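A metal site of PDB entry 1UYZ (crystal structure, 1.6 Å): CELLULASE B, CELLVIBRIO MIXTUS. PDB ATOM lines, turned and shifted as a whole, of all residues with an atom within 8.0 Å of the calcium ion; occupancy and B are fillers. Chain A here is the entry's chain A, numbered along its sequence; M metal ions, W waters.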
ATOM      1  N   GLN A  14      -4.567 -21.252  -4.976  1.00  0.00           N
ATOM      2  CA  GLN A  14      -5.269 -21.673  -3.772  1.00  0.00           C
ATOM      3  C   GLN A  14      -6.191 -20.582  -3.286  1.00  0.00           C
ATOM      4  O   GLN A  14      -6.082 -19.432  -3.718  1.00  0.00           O
ATOM      5  CB  GLN A  14      -4.276 -22.033  -2.685  1.00  0.00           C
ATOM      6  CG  GLN A  14      -3.564 -20.837  -2.020  1.00  0.00           C
ATOM      7  CD  GLN A  14      -4.399 -20.198  -0.916  1.00  0.00           C
ATOM      8  OE1 GLN A  14      -5.019 -20.886  -0.122  1.00  0.00           O
ATOM      9  NE2 GLN A  14      -4.410 -18.864  -0.887  1.00  0.00           N
ATOM     10  N   SER A  15      -7.078 -20.946  -2.371  1.00  0.00           N
ATOM     11  CA  SER A  15      -7.914 -19.976  -1.684  1.00  0.00           C
ATOM     12  C   SER A  15      -8.108 -20.384  -0.227  1.00  0.00           C
ATOM     13  O   SER A  15      -8.515 -21.518   0.066  1.00  0.00           O
ATOM     14  CB  SER A  15      -9.268 -19.852  -2.363  1.00  0.00           C
ATOM     15  OG  SER A  15     -10.067 -18.842  -1.724  1.00  0.00           O
ATOM     16  N   GLY A  16      -7.809 -19.460   0.673  1.00  0.00           N
ATOM     17  CA  GLY A  16      -8.146 -19.546   2.074  1.00  0.00           C
ATOM     18  C   GLY A  16      -7.207 -20.315   2.985  1.00  0.00           C
ATOM     19  O   GLY A  16      -7.492 -20.419   4.177  1.00  0.00           O
ATOM     20  N   THR A  17      -6.093 -20.827   2.465  1.00  0.00           N
ATOM     21  CA  THR A  17      -5.198 -21.683   3.234  1.00  0.00           C
ATOM     22  C   THR A  17      -3.837 -21.049   3.429  1.00  0.00           C
ATOM     23  O   THR A  17      -3.553 -19.991   2.885  1.00  0.00           O
ATOM     24  CB  THR A  17      -5.018 -23.065   2.579  1.00  0.00           C
ATOM     25  OG1 THR A  17      -4.207 -22.940   1.393  1.00  0.00           O
ATOM     26  CG2 THR A  17      -6.367 -23.632   2.104  1.00  0.00           C
ATOM     27  N   GLN A  18      -3.000 -21.733   4.190  1.00  0.00           N
ATOM     28  CA  GLN A  18      -1.670 -21.254   4.550  1.00  0.00           C
ATOM     29  C   GLN A  18      -0.745 -22.455   4.697  1.00  0.00           C
ATOM     30  O   GLN A  18      -1.138 -23.474   5.246  1.00  0.00           O
ATOM     31  CB  GLN A  18      -1.784 -20.468   5.867  1.00  0.00           C
ATOM     32  CG  GLN A  18      -0.514 -20.006   6.500  1.00  0.00           C
ATOM     33  CD  GLN A  18      -0.785 -18.912   7.524  1.00  0.00           C
ATOM     34  OE1 GLN A  18      -1.780 -18.978   8.258  1.00  0.00           O
ATOM     35  NE2 GLN A  18       0.076 -17.909   7.565  1.00  0.00           N
ATOM     36  N   GLY A  32      -2.320 -25.958   5.712  1.00  0.00           N
ATOM     37  CA  GLY A  32      -3.169 -25.873   6.893  1.00  0.00           C
ATOM     38  C   GLY A  32      -4.218 -24.788   6.757  1.00  0.00           C
ATOM     39  O   GLY A  32      -4.358 -24.181   5.696  1.00  0.00           O
ATOM     40  N   TYR A  33      -4.945 -24.531   7.843  1.00  0.00           N
ATOM     41  CA  TYR A  33      -6.000 -23.524   7.862  1.00  0.00           C
ATOM     42  C   TYR A  33      -7.030 -23.758   6.752  1.00  0.00           C
ATOM     43  O   TYR A  33      -7.392 -22.851   5.992  1.00  0.00           O
ATOM     44  CB  TYR A  33      -5.396 -22.104   7.808  1.00  0.00           C
ATOM     45  CG  TYR A  33      -4.509 -21.832   8.991  1.00  0.00           C
ATOM     46  CD1 TYR A  33      -3.209 -22.328   9.049  1.00  0.00           C
ATOM     47  CD2 TYR A  33      -4.987 -21.126  10.089  1.00  0.00           C
ATOM     48  CE1 TYR A  33      -2.404 -22.105  10.143  1.00  0.00           C
ATOM     49  CE2 TYR A  33      -4.185 -20.900  11.192  1.00  0.00           C
ATOM     50  CZ  TYR A  33      -2.901 -21.388  11.211  1.00  0.00           C
ATOM     51  OH  TYR A  33      -2.101 -21.174  12.307  1.00  0.00           O
ATOM     52  N   ILE A  34      -7.471 -25.003   6.653  1.00  0.00           N
ATOM     53  CA  ILE A  34      -8.423 -25.424   5.647  1.00  0.00           C
ATOM     54  C   ILE A  34      -9.806 -25.425   6.258  1.00  0.00           C
ATOM     55  O   ILE A  34     -10.040 -26.035   7.299  1.00  0.00           O
ATOM     56  CB  ILE A  34      -8.091 -26.834   5.134  1.00  0.00           C
ATOM     57  CG1 ILE A  34      -6.636 -26.890   4.656  1.00  0.00           C
ATOM     58  CG2 ILE A  34      -9.039 -27.204   3.992  1.00  0.00           C
ATOM     59  CD1 ILE A  34      -6.177 -28.270   4.183  1.00  0.00           C
ATOM     60  N   ASP A  35     -10.711 -24.700   5.608  1.00  0.00           N
ATOM     61  CA  ASP A  35     -12.086 -24.536   6.067  1.00  0.00           C
ATOM     62  C   ASP A  35     -13.043 -24.705   4.888  1.00  0.00           C
ATOM     63  O   ASP A  35     -12.637 -24.667   3.736  1.00  0.00           O
ATOM     64  CB  ASP A  35     -12.291 -23.145   6.638  1.00  0.00           C
ATOM     65  CG  ASP A  35     -11.261 -22.781   7.660  1.00  0.00           C
ATOM     66  OD1 ASP A  35     -11.552 -22.921   8.873  1.00  0.00           O
ATOM     67  OD2 ASP A  35     -10.150 -22.322   7.338  1.00  0.00           O
ATOM     68  N   ALA A  36     -14.333 -24.821   5.182  1.00  0.00           N
ATOM     69  CA  ALA A  36     -15.351 -24.965   4.142  1.00  0.00           C
ATOM     70  C   ALA A  36     -15.270 -23.812   3.129  1.00  0.00           C
ATOM     71  O   ALA A  36     -15.258 -22.646   3.513  1.00  0.00           O
ATOM     72  CB  ALA A  36     -16.734 -25.015   4.780  1.00  0.00           C
ATOM     73  N   GLY A  37     -15.184 -24.155   1.838  1.00  0.00           N
ATOM     74  CA  GLY A  37     -15.061 -23.182   0.778  1.00  0.00           C
ATOM     75  C   GLY A  37     -13.647 -23.078   0.225  1.00  0.00           C
ATOM     76  O   GLY A  37     -13.460 -22.715  -0.948  1.00  0.00           O
ATOM     77  N   ASP A  38     -12.654 -23.384   1.056  1.00  0.00           N
ATOM     78  CA  ASP A  38     -11.258 -23.290   0.654  1.00  0.00           C
ATOM     79  C   ASP A  38     -10.962 -24.321  -0.430  1.00  0.00           C
ATOM     80  O   ASP A  38     -11.633 -25.356  -0.545  1.00  0.00           O
ATOM     81  CB  ASP A  38     -10.329 -23.523   1.845  1.00  0.00           C
ATOM     82  CG  ASP A  38     -10.377 -22.410   2.871  1.00  0.00           C
ATOM     83  OD1 ASP A  38     -10.969 -21.342   2.587  1.00  0.00           O
ATOM     84  OD2 ASP A  38      -9.829 -22.524   3.999  1.00  0.00           O
ATOM     85  N   TRP A  39      -9.947 -24.029  -1.236  1.00  0.00           N
ATOM     86  CA  TRP A  39      -9.561 -24.944  -2.295  1.00  0.00           C
ATOM     87  C   TRP A  39      -8.095 -24.831  -2.698  1.00  0.00           C
ATOM     88  O   TRP A  39      -7.424 -23.858  -2.400  1.00  0.00           O
ATOM     89  CB  TRP A  39     -10.470 -24.746  -3.513  1.00  0.00           C
ATOM     90  CG  TRP A  39     -10.571 -23.355  -4.065  1.00  0.00           C
ATOM     91  CD1 TRP A  39     -11.566 -22.439  -3.806  1.00  0.00           C
ATOM     92  CD2 TRP A  39      -9.691 -22.720  -4.997  1.00  0.00           C
ATOM     93  NE1 TRP A  39     -11.353 -21.291  -4.527  1.00  0.00           N
ATOM     94  CE2 TRP A  39     -10.205 -21.436  -5.272  1.00  0.00           C
ATOM     95  CE3 TRP A  39      -8.514 -23.111  -5.641  1.00  0.00           C
ATOM     96  CZ2 TRP A  39      -9.578 -20.542  -6.146  1.00  0.00           C
ATOM     97  CZ3 TRP A  39      -7.903 -22.233  -6.513  1.00  0.00           C
ATOM     98  CH2 TRP A  39      -8.429 -20.959  -6.756  1.00  0.00           C
ATOM     99  N   ALA A 115     -12.458 -28.085  -0.151  1.00  0.00           N
ATOM    100  CA  ALA A 115     -12.816 -28.490   1.213  1.00  0.00           C
ATOM    101  C   ALA A 115     -14.288 -28.215   1.461  1.00  0.00           C
ATOM    102  O   ALA A 115     -14.757 -27.089   1.315  1.00  0.00           O
ATOM    103  CB  ALA A 115     -11.966 -27.756   2.230  1.00  0.00           C
ATOM    104  N   GLY A 118     -13.836 -28.113   7.186  1.00  0.00           N
ATOM    105  CA  GLY A 118     -12.468 -27.923   7.621  1.00  0.00           C
ATOM    106  C   GLY A 118     -12.075 -28.819   8.763  1.00  0.00           C
ATOM    107  O   GLY A 118     -12.739 -29.816   9.058  1.00  0.00           O
HETATM  108 CA    CA M   1      -8.979 -21.215   5.673  1.00  0.00          CA
HETATM  109  O   HOH W   1      -8.573 -19.864   7.577  1.00  0.00           O
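The backbone NH (N) of Gly 16 lies within hydrogen-bond range of the side-chain amide oxygen (OE1) of Gln 14 (3.2 Å). O of Asp 38 is in hydrogen-bond range of N of Ala 115 (2.9 Å).
O of Gly 16 is bound to the calcium ion, at 2.3 Å. OD2 of Asp 38 binds the calcium ion, 2.3 Å away. O of Tyr 33 is bound to the calcium ion. OD2 of Asp 35 is bound to the calcium ion, 2.3 Å away. Water W1 binds the calcium ion, 2.4 Å away.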
